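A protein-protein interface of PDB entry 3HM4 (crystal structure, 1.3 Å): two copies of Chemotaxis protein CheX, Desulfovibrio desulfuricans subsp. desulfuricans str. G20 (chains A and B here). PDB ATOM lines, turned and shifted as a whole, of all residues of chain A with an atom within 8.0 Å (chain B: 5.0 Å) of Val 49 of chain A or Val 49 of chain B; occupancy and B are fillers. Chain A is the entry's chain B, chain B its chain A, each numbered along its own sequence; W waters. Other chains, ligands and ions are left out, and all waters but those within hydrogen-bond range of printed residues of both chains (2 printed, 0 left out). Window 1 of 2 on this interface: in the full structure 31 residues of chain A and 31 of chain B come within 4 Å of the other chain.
Water W1 lies within hydrogen-bond range of the side-chain hydroxyl of Thr 118 of chain A (2.7 Å), a ring nitrogen (ND1) of His 131 of chain B (2.8 Å) and the backbone carbonyl oxygen of Pro 119 of chain A (2.8 Å).
Water W2 lies within hydrogen-bond range of the side-chain hydroxyl of Thr 118 of chain B, a ring nitrogen (ND1) of His 131 of chain A and the backbone carbonyl oxygen of Pro 119 of chain B.
Val 49 of chain A touches its own counterpart, Val 49 of chain B.
Val 49 of chain A touches Ser 120 of chain B, and with the chains exchanged Ser 120 of chain A touches Val 49 of chain B.
Ser 120 of chain A touches Ile 129 of chain B, and with the chains exchanged Ile 129 of chain A touches Ser 120 of chain B.
Ile 122 of chain B touches its own counterpart, Ile 122 of chain A.
Of the 18 pairs that touch across the chains among the printed residues, 12 have their exchanged pair printed and touching as well.
Val 49 of chain A touches two residues of chain B.
Printed residues of chain B within 4 Å of Thr 118 of chain A: Ser 59 (3.5 Å).
Of the printed residues of chain B, Ser 120 of chain A touches Val 49, Ile 129 and His 131.
Of the printed residues of chain B, Ile 122 of chain A touches Ile 122.
No residue of chain A comes within 4 Å of Ala 48 of chain B.
Val 49 of chain B touches two residues of chain A.
The nearest printed residue of chain A that does not touch Thr 118 of chain B is Ile 52 of chain A (4.9 Å).
Hydrophobic or aromatic side chains of chain B within 4 Å of the printed part of chain A: Val 49, Pro 119, Ile 122, Ile 129 and His 131.
OG1 of Thr 118 of chain B lies close to O of Gly 58 of chain A (3.3 Å).
The backbone carbonyl oxygen of Pro 119 of chain B is in hydrogen-bond range of the backbone NH of Val 132 of chain A, 2.9 Å away.
A ring nitrogen (ND1) of His 131 of chain A lies within hydrogen-bond range of the side-chain hydroxyl (OG) of Ser 120 of chain B (3.5 Å).
Among the printed residues, pairs that only touch across the chains: Ser 130 of chain A with Ser 120 of chain B (3.1 Å), Val 121 of chain A with Ile 129 of chain B (3.4 Å), Ala 117 of chain A with Gly 51 of chain B (3.4 Å), Ser 59 of chain A with Thr 118 of chain B (3.5 Å), Thr 118 of chain A with Ser 59 of chain B (3.5 Å), Ser 120 of chain A with His 131 of chain B (3.5 Å), Val 132 of chain A with Thr 118 of chain B (3.6 Å), Val 49 of chain A with Ser 120 of chain B (3.6 Å), Ser 120 of chain A with Val 49 of chain B (3.7 Å), Ile 122 of chain A with Ile 122 of chain B (3.7 Å), Val 49 of chain A with Val 49 of chain B (3.8 Å), Pro 119 of chain A with His 131 of chain B (3.8 Å), His 131 of chain A with Pro 119 of chain B (3.9 Å), Ile 129 of chain A with Ser 120 of chain B (3.9 Å) and Ser 120 of chain A with Ile 129 of chain B (3.9 Å).
The backbone NH of Ile 122 of chain B sits at hydrogen-bond distance from the backbone carbonyl oxygen of Ser 47 of chain B, 2.7 Å away.
The side-chain hydroxyl (OG) of Ser 59 of chain B is in hydrogen-bond range of the backbone carbonyl oxygen (O) of Val 50 of chain B.
The backbone NH (N) of Ile 122 of chain A is in hydrogen-bond range of the backbone carbonyl oxygen (O) of Ser 47 of chain A (2.8 Å).
The backbone NH (N) of Ser 120 of chain A is in hydrogen-bond range of the backbone carbonyl oxygen (O) of Val 49 of chain A.
The backbone carbonyl oxygen (O) of Gly 51 of chain A sits at hydrogen-bond distance from the backbone NH (N) of Ala 117 of chain A (2.9 Å).
N of Gly 58 of chain A lies within hydrogen-bond range of O of Ile 52 of chain A (2.9 Å).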
ATOM      1  N   SER A  47     -18.917 -27.579  29.488  1.00  0.00           N
ATOM      2  CA  SER A  47     -19.471 -26.253  29.601  1.00  0.00           C
ATOM      3  C   SER A  47     -20.933 -26.249  29.185  1.00  0.00           C
ATOM      4  O   SER A  47     -21.445 -27.159  28.549  1.00  0.00           O
ATOM      5  CB  SER A  47     -18.725 -25.236  28.740  1.00  0.00           C
ATOM      6  OG  SER A  47     -17.355 -25.115  29.129  1.00  0.00           O
ATOM      7  N   ALA A  48     -21.617 -25.189  29.592  1.00  0.00           N
ATOM      8  CA  ALA A  48     -22.939 -24.911  29.072  1.00  0.00           C
ATOM      9  C   ALA A  48     -23.057 -23.415  28.869  1.00  0.00           C
ATOM     10  O   ALA A  48     -22.378 -22.639  29.549  1.00  0.00           O
ATOM     11  CB  ALA A  48     -24.049 -25.431  29.972  1.00  0.00           C
ATOM     12  N   VAL A  49     -23.898 -23.022  27.926  1.00  0.00           N
ATOM     13  CA  VAL A  49     -24.047 -21.612  27.569  1.00  0.00           C
ATOM     14  C   VAL A  49     -25.489 -21.349  27.171  1.00  0.00           C
ATOM     15  O   VAL A  49     -26.113 -22.189  26.526  1.00  0.00           O
ATOM     16  CB  VAL A  49     -23.043 -21.191  26.509  1.00  0.00           C
ATOM     17  CG1 VAL A  49     -23.188 -21.994  25.208  1.00  0.00           C
ATOM     18  CG2 VAL A  49     -23.094 -19.675  26.282  1.00  0.00           C
ATOM     19  N   VAL A  50     -25.994 -20.184  27.579  1.00  0.00           N
ATOM     20  CA  VAL A  50     -27.348 -19.794  27.250  1.00  0.00           C
ATOM     21  C   VAL A  50     -27.433 -18.291  27.042  1.00  0.00           C
ATOM     22  O   VAL A  50     -26.951 -17.511  27.846  1.00  0.00           O
ATOM     23  CB  VAL A  50     -28.333 -20.265  28.341  1.00  0.00           C
ATOM     24  CG1 VAL A  50     -28.010 -19.664  29.730  1.00  0.00           C
ATOM     25  CG2 VAL A  50     -29.800 -20.032  27.911  1.00  0.00           C
ATOM     26  N   GLY A  51     -27.996 -17.917  25.909  1.00  0.00           N
ATOM     27  CA  GLY A  51     -28.143 -16.524  25.561  1.00  0.00           C
ATOM     28  C   GLY A  51     -29.302 -15.847  26.287  1.00  0.00           C
ATOM     29  O   GLY A  51     -30.290 -16.482  26.637  1.00  0.00           O
ATOM     30  N   ILE A  52     -29.154 -14.548  26.481  1.00  0.00           N
ATOM     31  CA  ILE A  52     -30.180 -13.714  27.084  1.00  0.00           C
ATOM     32  C   ILE A  52     -30.356 -12.443  26.242  1.00  0.00           C
ATOM     33  O   ILE A  52     -29.428 -11.988  25.574  1.00  0.00           O
ATOM     34  CB  ILE A  52     -29.901 -13.437  28.605  1.00  0.00           C
ATOM     35  CG1 ILE A  52     -28.656 -12.570  28.828  1.00  0.00           C
ATOM     36  CG2 ILE A  52     -29.911 -14.763  29.365  1.00  0.00           C
ATOM     37  CD1 ILE A  52     -28.324 -12.229  30.304  1.00  0.00           C
ATOM     38  N   GLY A  58     -26.866 -10.676  25.664  1.00  0.00           N
ATOM     39  CA  GLY A  58     -25.746 -11.250  26.338  1.00  0.00           C
ATOM     40  C   GLY A  58     -25.830 -12.746  26.456  1.00  0.00           C
ATOM     41  O   GLY A  58     -26.529 -13.397  25.696  1.00  0.00           O
ATOM     42  N   SER A  59     -25.093 -13.277  27.419  1.00  0.00           N
ATOM     43  CA  SER A  59     -24.956 -14.685  27.586  1.00  0.00           C
ATOM     44  C   SER A  59     -24.481 -15.030  28.980  1.00  0.00           C
ATOM     45  O   SER A  59     -23.838 -14.228  29.639  1.00  0.00           O
ATOM     46  CB  SER A  59     -23.959 -15.183  26.565  1.00  0.00           C
ATOM     47  OG  SER A  59     -23.852 -16.600  26.608  1.00  0.00           O
ATOM     48  N   ILE A  60     -24.848 -16.251  29.417  1.00  0.00           N
ATOM     49  CA  ILE A  60     -24.424 -16.846  30.658  1.00  0.00           C
ATOM     50  C   ILE A  60     -23.777 -18.167  30.305  1.00  0.00           C
ATOM     51  O   ILE A  60     -24.375 -18.953  29.576  1.00  0.00           O
ATOM     52  CB  ILE A  60     -25.558 -17.137  31.623  1.00  0.00           C
ATOM     53  CG1 ILE A  60     -26.459 -15.931  31.830  1.00  0.00           C
ATOM     54  CG2 ILE A  60     -24.992 -17.618  32.961  1.00  0.00           C
ATOM     55  CD1 ILE A  60     -27.788 -16.270  32.543  1.00  0.00           C
ATOM     56  N   SER A  61     -22.558 -18.418  30.771  1.00  0.00           N
ATOM     57  CA  SER A  61     -21.936 -19.716  30.617  1.00  0.00           C
ATOM     58  C   SER A  61     -21.434 -20.251  31.926  1.00  0.00           C
ATOM     59  O   SER A  61     -21.214 -19.516  32.887  1.00  0.00           O
ATOM     60  CB  SER A  61     -20.805 -19.683  29.594  1.00  0.00           C
ATOM     61  OG  SER A  61     -19.756 -18.860  30.034  1.00  0.00           O
ATOM     62  N   VAL A  62     -21.253 -21.567  31.941  1.00  0.00           N
ATOM     63  CA  VAL A  62     -20.639 -22.254  33.070  1.00  0.00           C
ATOM     64  C   VAL A  62     -19.636 -23.258  32.509  1.00  0.00           C
ATOM     65  O   VAL A  62     -19.948 -23.990  31.574  1.00  0.00           O
ATOM     66  CB  VAL A  62     -21.651 -22.926  34.027  1.00  0.00           C
ATOM     67  CG1 VAL A  62     -22.569 -23.935  33.306  1.00  0.00           C
ATOM     68  CG2 VAL A  62     -20.898 -23.604  35.178  1.00  0.00           C
ATOM     69  N   THR A  63     -18.423 -23.243  33.041  1.00  0.00           N
ATOM     70  CA  THR A  63     -17.356 -24.160  32.610  1.00  0.00           C
ATOM     71  C   THR A  63     -16.875 -24.933  33.823  1.00  0.00           C
ATOM     72  O   THR A  63     -16.393 -24.341  34.809  1.00  0.00           O
ATOM     73  CB  THR A  63     -16.238 -23.407  31.882  1.00  0.00           C
ATOM     74  OG1 THR A  63     -16.786 -22.822  30.677  1.00  0.00           O
ATOM     75  CG2 THR A  63     -15.037 -24.334  31.550  1.00  0.00           C
ATOM     76  N   VAL A  92     -26.775 -31.155  33.072  1.00  0.00           N
ATOM     77  CA  VAL A  92     -26.176 -29.828  32.970  1.00  0.00           C
ATOM     78  C   VAL A  92     -27.121 -28.883  32.224  1.00  0.00           C
ATOM     79  O   VAL A  92     -27.200 -27.679  32.537  1.00  0.00           O
ATOM     80  CB  VAL A  92     -24.766 -29.888  32.369  1.00  0.00           C
ATOM     81  CG1 VAL A  92     -24.193 -28.459  32.185  1.00  0.00           C
ATOM     82  CG2 VAL A  92     -23.865 -30.690  33.295  1.00  0.00           C
ATOM     83  N   GLY A  93     -27.838 -29.394  31.226  1.00  0.00           N
ATOM     84  CA  GLY A  93     -28.841 -28.569  30.528  1.00  0.00           C
ATOM     85  C   GLY A  93     -29.905 -28.019  31.446  1.00  0.00           C
ATOM     86  O   GLY A  93     -30.266 -26.823  31.355  1.00  0.00           O
ATOM     87  N   THR A  96     -28.513 -25.351  33.755  1.00  0.00           N
ATOM     88  CA  THR A  96     -28.313 -24.114  33.019  1.00  0.00           C
ATOM     89  C   THR A  96     -29.639 -23.387  32.783  1.00  0.00           C
ATOM     90  O   THR A  96     -29.708 -22.159  32.920  1.00  0.00           O
ATOM     91  CB  THR A  96     -27.511 -24.384  31.739  1.00  0.00           C
ATOM     92  OG1 THR A  96     -26.283 -25.010  32.118  1.00  0.00           O
ATOM     93  CG2 THR A  96     -27.151 -23.088  31.033  1.00  0.00           C
ATOM     94  N   ASN A  97     -30.657 -24.129  32.375  1.00  0.00           N
ATOM     95  CA  ASN A  97     -32.014 -23.564  32.261  1.00  0.00           C
ATOM     96  C   ASN A  97     -32.472 -22.892  33.557  1.00  0.00           C
ATOM     97  O   ASN A  97     -33.006 -21.777  33.549  1.00  0.00           O
ATOM     98  CB  ASN A  97     -33.058 -24.594  31.781  1.00  0.00           C
ATOM     99  CG  ASN A  97     -33.307 -24.548  30.291  1.00  0.00           C
ATOM    100  OD1 ASN A  97     -33.384 -23.458  29.709  1.00  0.00           O
ATOM    101  ND2 ASN A  97     -33.471 -25.725  29.680  1.00  0.00           N
ATOM    102  N   SER A 100     -30.401 -19.723  34.366  1.00  0.00           N
ATOM    103  CA  SER A 100     -30.922 -18.636  33.530  1.00  0.00           C
ATOM    104  C   SER A 100     -32.232 -18.065  34.111  1.00  0.00           C
ATOM    105  O   SER A 100     -32.391 -16.872  34.279  1.00  0.00           O
ATOM    106  CB  SER A 100     -31.177 -19.124  32.092  1.00  0.00           C
ATOM    107  OG  SER A 100     -31.805 -18.108  31.323  1.00  0.00           O
ATOM    108  N   ALA A 117     -32.822 -17.754  26.025  1.00  0.00           N
ATOM    109  CA  ALA A 117     -32.773 -18.711  24.919  1.00  0.00           C
ATOM    110  C   ALA A 117     -32.643 -20.146  25.450  1.00  0.00           C
ATOM    111  O   ALA A 117     -32.659 -20.388  26.659  1.00  0.00           O
ATOM    112  CB  ALA A 117     -31.603 -18.299  23.975  1.00  0.00           C
ATOM    113  N   THR A 118     -32.528 -21.123  24.552  1.00  0.00           N
ATOM    114  CA  THR A 118     -32.318 -22.507  24.968  1.00  0.00           C
ATOM    115  C   THR A 118     -30.809 -22.738  25.192  1.00  0.00           C
ATOM    116  O   THR A 118     -29.996 -22.243  24.427  1.00  0.00           O
ATOM    117  CB  THR A 118     -32.824 -23.489  23.886  1.00  0.00           C
ATOM    118  OG1 THR A 118     -32.337 -23.132  22.601  1.00  0.00           O
ATOM    119  CG2 THR A 118     -34.345 -23.417  23.843  1.00  0.00           C
ATOM    120  N   PRO A 119     -30.432 -23.507  26.236  1.00  0.00           N
ATOM    121  CA  PRO A 119     -29.012 -23.746  26.444  1.00  0.00           C
ATOM    122  C   PRO A 119     -28.399 -24.729  25.448  1.00  0.00           C
ATOM    123  O   PRO A 119     -29.119 -25.475  24.782  1.00  0.00           O
ATOM    124  CB  PRO A 119     -28.944 -24.383  27.847  1.00  0.00           C
ATOM    125  CG  PRO A 119     -30.295 -24.018  28.513  1.00  0.00           C
ATOM    126  CD  PRO A 119     -31.241 -24.044  27.334  1.00  0.00           C
ATOM    127  N   SER A 120     -27.072 -24.700  25.391  1.00  0.00           N
ATOM    128  CA  SER A 120     -26.279 -25.749  24.733  1.00  0.00           C
ATOM    129  C   SER A 120     -25.257 -26.260  25.716  1.00  0.00           C
ATOM    130  O   SER A 120     -24.746 -25.501  26.522  1.00  0.00           O
ATOM    131  CB  SER A 120     -25.604 -25.292  23.447  1.00  0.00           C
ATOM    132  OG  SER A 120     -26.544 -25.087  22.428  1.00  0.00           O
ATOM    133  N   VAL A 121     -24.959 -27.571  25.658  1.00  0.00           N
ATOM    134  CA  VAL A 121     -23.952 -28.221  26.508  1.00  0.00           C
ATOM    135  C   VAL A 121     -22.798 -28.671  25.596  1.00  0.00           C
ATOM    136  O   VAL A 121     -22.996 -29.256  24.544  1.00  0.00           O
ATOM    137  CB  VAL A 121     -24.530 -29.381  27.296  1.00  0.00           C
ATOM    138  CG1 VAL A 121     -23.462 -30.189  28.022  1.00  0.00           C
ATOM    139  CG2 VAL A 121     -25.652 -28.856  28.262  1.00  0.00           C
ATOM    140  N   ILE A 122     -21.596 -28.355  26.051  1.00  0.00           N
ATOM    141  CA  ILE A 122     -20.346 -28.618  25.347  1.00  0.00           C
ATOM    142  C   ILE A 122     -19.524 -29.627  26.110  1.00  0.00           C
ATOM    143  O   ILE A 122     -19.342 -29.500  27.329  1.00  0.00           O
ATOM    144  CB  ILE A 122     -19.531 -27.338  25.168  1.00  0.00           C
ATOM    145  CG1 ILE A 122     -20.334 -26.292  24.347  1.00  0.00           C
ATOM    146  CG2 ILE A 122     -18.237 -27.635  24.443  1.00  0.00           C
ATOM    147  CD1 ILE A 122     -21.093 -25.349  25.058  1.00  0.00           C
ATOM    148  N   ILE A 129     -14.277 -22.091  25.545  1.00  0.00           N
ATOM    149  CA  ILE A 129     -15.429 -21.288  25.178  1.00  0.00           C
ATOM    150  C   ILE A 129     -15.033 -19.820  25.296  1.00  0.00           C
ATOM    151  O   ILE A 129     -14.396 -19.414  26.286  1.00  0.00           O
ATOM    152  CB  ILE A 129     -16.688 -21.609  26.030  1.00  0.00           C
ATOM    153  CG1 ILE A 129     -17.905 -20.787  25.537  1.00  0.00           C
ATOM    154  CG2 ILE A 129     -16.429 -21.442  27.504  1.00  0.00           C
ATOM    155  CD1 ILE A 129     -19.273 -21.287  26.055  1.00  0.00           C
ATOM    156  N   SER A 130     -15.449 -19.043  24.302  1.00  0.00           N
ATOM    157  CA  SER A 130     -15.178 -17.624  24.229  1.00  0.00           C
ATOM    158  C   SER A 130     -16.484 -16.880  23.951  1.00  0.00           C
ATOM    159  O   SER A 130     -17.171 -17.214  23.016  1.00  0.00           O
ATOM    160  CB  SER A 130     -14.223 -17.322  23.063  1.00  0.00           C
ATOM    161  OG  SER A 130     -12.968 -18.003  23.175  1.00  0.00           O
ATOM    162  N   HIS A 131     -16.742 -15.841  24.723  1.00  0.00           N
ATOM    163  CA  HIS A 131     -17.865 -14.941  24.485  1.00  0.00           C
ATOM    164  C   HIS A 131     -17.503 -13.882  23.460  1.00  0.00           C
ATOM    165  O   HIS A 131     -16.447 -13.246  23.560  1.00  0.00           O
ATOM    166  CB  HIS A 131     -18.311 -14.266  25.787  1.00  0.00           C
ATOM    167  CG  HIS A 131     -18.970 -15.226  26.713  1.00  0.00           C
ATOM    168  ND1 HIS A 131     -20.318 -15.479  26.632  1.00  0.00           N
ATOM    169  CD2 HIS A 131     -18.493 -15.978  27.739  1.00  0.00           C
ATOM    170  CE1 HIS A 131     -20.639 -16.375  27.555  1.00  0.00           C
ATOM    171  NE2 HIS A 131     -19.547 -16.701  28.232  1.00  0.00           N
ATOM    172  N   VAL A 132     -18.371 -13.684  22.483  1.00  0.00           N
ATOM    173  CA  VAL A 132     -18.174 -12.756  21.370  1.00  0.00           C
ATOM    174  C   VAL A 132     -18.963 -11.494  21.680  1.00  0.00           C
ATOM    175  O   VAL A 132     -20.182 -11.440  21.558  1.00  0.00           O
ATOM    176  CB  VAL A 132     -18.614 -13.357  20.049  1.00  0.00           C
ATOM    177  CG1 VAL A 132     -18.513 -12.383  18.880  1.00  0.00           C
ATOM    178  CG2 VAL A 132     -17.865 -14.650  19.780  1.00  0.00           C
ATOM    179  N   GLU A 152     -19.544 -17.371  33.781  1.00  0.00           N
ATOM    180  CA  GLU A 152     -19.189 -16.139  33.089  1.00  0.00           C
ATOM    181  C   GLU A 152     -20.431 -15.554  32.480  1.00  0.00           C
ATOM    182  O   GLU A 152     -21.378 -16.263  32.116  1.00  0.00           O
ATOM    183  CB  GLU A 152     -18.149 -16.396  31.985  1.00  0.00           C
ATOM    184  CG  GLU A 152     -16.884 -17.027  32.526  1.00  0.00           C
ATOM    185  CD  GLU A 152     -15.829 -17.250  31.469  1.00  0.00           C
ATOM    186  OE1 GLU A 152     -16.153 -17.646  30.322  1.00  0.00           O
ATOM    187  OE2 GLU A 152     -14.659 -17.147  31.808  1.00  0.00           O
ATOM    188  N   SER B  47     -16.899 -24.676  16.841  1.00  0.00           N
ATOM    189  CA  SER B  47     -18.321 -24.431  16.774  1.00  0.00           C
ATOM    190  C   SER B  47     -18.608 -23.022  17.253  1.00  0.00           C
ATOM    191  O   SER B  47     -17.810 -22.410  17.964  1.00  0.00           O
ATOM    192  CB  SER B  47     -19.122 -25.406  17.624  1.00  0.00           C
ATOM    193  OG  SER B  47     -18.959 -26.758  17.205  1.00  0.00           O
ATOM    194  N   ALA B  48     -19.793 -22.553  16.898  1.00  0.00           N
ATOM    195  CA  ALA B  48     -20.320 -21.308  17.450  1.00  0.00           C
ATOM    196  C   ALA B  48     -21.792 -21.504  17.702  1.00  0.00           C
ATOM    197  O   ALA B  48     -22.441 -22.294  17.013  1.00  0.00           O
ATOM    198  CB  ALA B  48     -20.059 -20.118  16.569  1.00  0.00           C
ATOM    199  N   VAL B  49     -22.321 -20.767  18.667  1.00  0.00           N
ATOM    200  CA  VAL B  49     -23.711 -20.900  19.039  1.00  0.00           C
ATOM    201  C   VAL B  49     -24.241 -19.565  19.488  1.00  0.00           C
ATOM    202  O   VAL B  49     -23.517 -18.803  20.139  1.00  0.00           O
ATOM    203  CB  VAL B  49     -23.919 -22.012  20.102  1.00  0.00           C
ATOM    204  CG1 VAL B  49     -23.158 -21.740  21.393  1.00  0.00           C
ATOM    205  CG2 VAL B  49     -25.404 -22.265  20.367  1.00  0.00           C
ATOM    206  N   VAL B  50     -25.512 -19.307  19.187  1.00  0.00           N
ATOM    207  CA  VAL B  50     -26.153 -18.041  19.534  1.00  0.00           C
ATOM    208  C   VAL B  50     -27.620 -18.260  19.805  1.00  0.00           C
ATOM    209  O   VAL B  50     -28.317 -18.847  18.997  1.00  0.00           O
ATOM    210  CB  VAL B  50     -25.913 -16.931  18.455  1.00  0.00           C
ATOM    211  CG1 VAL B  50     -26.501 -17.278  17.041  1.00  0.00           C
ATOM    212  CG2 VAL B  50     -26.420 -15.577  18.957  1.00  0.00           C
ATOM    213  N   GLY B  51     -28.065 -17.771  20.961  1.00  0.00           N
ATOM    214  CA  GLY B  51     -29.462 -17.930  21.332  1.00  0.00           C
ATOM    215  C   GLY B  51     -30.363 -16.898  20.670  1.00  0.00           C
ATOM    216  O   GLY B  51     -29.934 -15.780  20.350  1.00  0.00           O
ATOM    217  N   SER B  59     -32.113 -21.534  19.432  1.00  0.00           N
ATOM    218  CA  SER B  59     -30.695 -21.330  19.229  1.00  0.00           C
ATOM    219  C   SER B  59     -30.301 -21.679  17.794  1.00  0.00           C
ATOM    220  O   SER B  59     -30.978 -22.471  17.142  1.00  0.00           O
ATOM    221  CB  SER B  59     -29.965 -22.265  20.163  1.00  0.00           C
ATOM    222  OG  SER B  59     -28.579 -22.094  20.105  1.00  0.00           O
ATOM    223  N   ILE B  60     -29.219 -21.052  17.345  1.00  0.00           N
ATOM    224  CA  ILE B  60     -28.574 -21.376  16.067  1.00  0.00           C
ATOM    225  C   ILE B  60     -27.126 -21.754  16.385  1.00  0.00           C
ATOM    226  O   ILE B  60     -26.441 -21.026  17.122  1.00  0.00           O
ATOM    227  CB  ILE B  60     -28.564 -20.192  15.074  1.00  0.00           C
ATOM    228  CG1 ILE B  60     -29.955 -19.579  14.916  1.00  0.00           C
ATOM    229  CG2 ILE B  60     -27.946 -20.603  13.711  1.00  0.00           C
ATOM    230  CD1 ILE B  60     -29.947 -18.219  14.214  1.00  0.00           C
ATOM    231  N   SER B  61     -26.661 -22.898  15.878  1.00  0.00           N
ATOM    232  CA  SER B  61     -25.244 -23.243  16.000  1.00  0.00           C
ATOM    233  C   SER B  61     -24.657 -23.607  14.651  1.00  0.00           C
ATOM    234  O   SER B  61     -25.353 -23.954  13.705  1.00  0.00           O
ATOM    235  CB  SER B  61     -25.007 -24.382  17.001  1.00  0.00           C
ATOM    236  OG  SER B  61     -25.612 -25.560  16.552  1.00  0.00           O
ATOM    237  N   THR B  96     -21.111 -15.658  12.945  1.00  0.00           N
ATOM    238  CA  THR B  96     -22.290 -16.082  13.712  1.00  0.00           C
ATOM    239  C   THR B  96     -23.254 -14.941  14.017  1.00  0.00           C
ATOM    240  O   THR B  96     -24.475 -15.104  13.901  1.00  0.00           O
ATOM    241  CB  THR B  96     -21.859 -16.838  14.962  1.00  0.00           C
ATOM    242  OG1 THR B  96     -20.968 -17.911  14.600  1.00  0.00           O
ATOM    243  CG2 THR B  96     -23.035 -17.395  15.743  1.00  0.00           C
ATOM    244  N   THR B 118     -25.712 -12.750  22.399  1.00  0.00           N
ATOM    245  CA  THR B 118     -24.316 -12.678  21.942  1.00  0.00           C
ATOM    246  C   THR B 118     -23.820 -14.113  21.663  1.00  0.00           C
ATOM    247  O   THR B 118     -24.131 -15.048  22.427  1.00  0.00           O
ATOM    248  CB  THR B 118     -23.421 -11.977  22.994  1.00  0.00           C
ATOM    249  OG1 THR B 118     -23.618 -12.589  24.275  1.00  0.00           O
ATOM    250  CG2 THR B 118     -23.731 -10.469  23.064  1.00  0.00           C
ATOM    251  N   PRO B 119     -23.056 -14.305  20.577  1.00  0.00           N
ATOM    252  CA  PRO B 119     -22.536 -15.651  20.315  1.00  0.00           C
ATOM    253  C   PRO B 119     -21.418 -16.071  21.260  1.00  0.00           C
ATOM    254  O   PRO B 119     -20.780 -15.251  21.902  1.00  0.00           O
ATOM    255  CB  PRO B 119     -21.976 -15.553  18.874  1.00  0.00           C
ATOM    256  CG  PRO B 119     -22.570 -14.297  18.322  1.00  0.00           C
ATOM    257  CD  PRO B 119     -22.736 -13.374  19.475  1.00  0.00           C
ATOM    258  N   SER B 120     -21.189 -17.381  21.259  1.00  0.00           N
ATOM    259  CA  SER B 120     -19.994 -17.970  21.862  1.00  0.00           C
ATOM    260  C   SER B 120     -19.342 -18.876  20.825  1.00  0.00           C
ATOM    261  O   SER B 120     -20.025 -19.486  19.990  1.00  0.00           O
ATOM    262  CB  SER B 120     -20.272 -18.772  23.138  1.00  0.00           C
ATOM    263  OG  SER B 120     -20.685 -17.924  24.197  1.00  0.00           O
ATOM    264  N   ILE B 122     -16.602 -22.074  20.380  1.00  0.00           N
ATOM    265  CA  ILE B 122     -16.056 -23.231  21.041  1.00  0.00           C
ATOM    266  C   ILE B 122     -14.923 -23.813  20.203  1.00  0.00           C
ATOM    267  O   ILE B 122     -15.051 -23.976  18.990  1.00  0.00           O
ATOM    268  CB  ILE B 122     -17.136 -24.308  21.268  1.00  0.00           C
ATOM    269  CG1 ILE B 122     -18.248 -23.763  22.206  1.00  0.00           C
ATOM    270  CG2 ILE B 122     -16.558 -25.598  21.883  1.00  0.00           C
ATOM    271  CD1 ILE B 122     -19.335 -23.130  21.559  1.00  0.00           C
ATOM    272  N   ILE B 129     -21.253 -30.410  20.813  1.00  0.00           N
ATOM    273  CA  ILE B 129     -22.237 -29.430  21.226  1.00  0.00           C
ATOM    274  C   ILE B 129     -23.607 -30.077  21.092  1.00  0.00           C
ATOM    275  O   ILE B 129     -23.908 -30.728  20.080  1.00  0.00           O
ATOM    276  CB  ILE B 129     -22.105 -28.098  20.464  1.00  0.00           C
ATOM    277  CG1 ILE B 129     -23.155 -27.074  20.931  1.00  0.00           C
ATOM    278  CG2 ILE B 129     -22.207 -28.279  18.984  1.00  0.00           C
ATOM    279  CD1 ILE B 129     -22.778 -25.584  20.617  1.00  0.00           C
ATOM    280  N   HIS B 131     -27.826 -29.238  21.853  1.00  0.00           N
ATOM    281  CA  HIS B 131     -28.926 -28.322  22.137  1.00  0.00           C
ATOM    282  C   HIS B 131     -29.845 -28.892  23.187  1.00  0.00           C
ATOM    283  O   HIS B 131     -30.252 -30.056  23.097  1.00  0.00           O
ATOM    284  CB  HIS B 131     -29.719 -27.990  20.866  1.00  0.00           C
ATOM    285  CG  HIS B 131     -28.944 -27.143  19.921  1.00  0.00           C
ATOM    286  ND1 HIS B 131     -28.973 -25.764  19.976  1.00  0.00           N
ATOM    287  CD2 HIS B 131     -28.142 -27.467  18.872  1.00  0.00           C
ATOM    288  CE1 HIS B 131     -28.178 -25.274  19.040  1.00  0.00           C
ATOM    289  NE2 HIS B 131     -27.649 -26.289  18.370  1.00  0.00           N
HETATM  290  O   HOH W   1     -30.318 -24.872  22.284  1.00  0.00           O
HETATM  291  O   HOH W   2     -21.536 -14.291  24.426  1.00  0.00           O
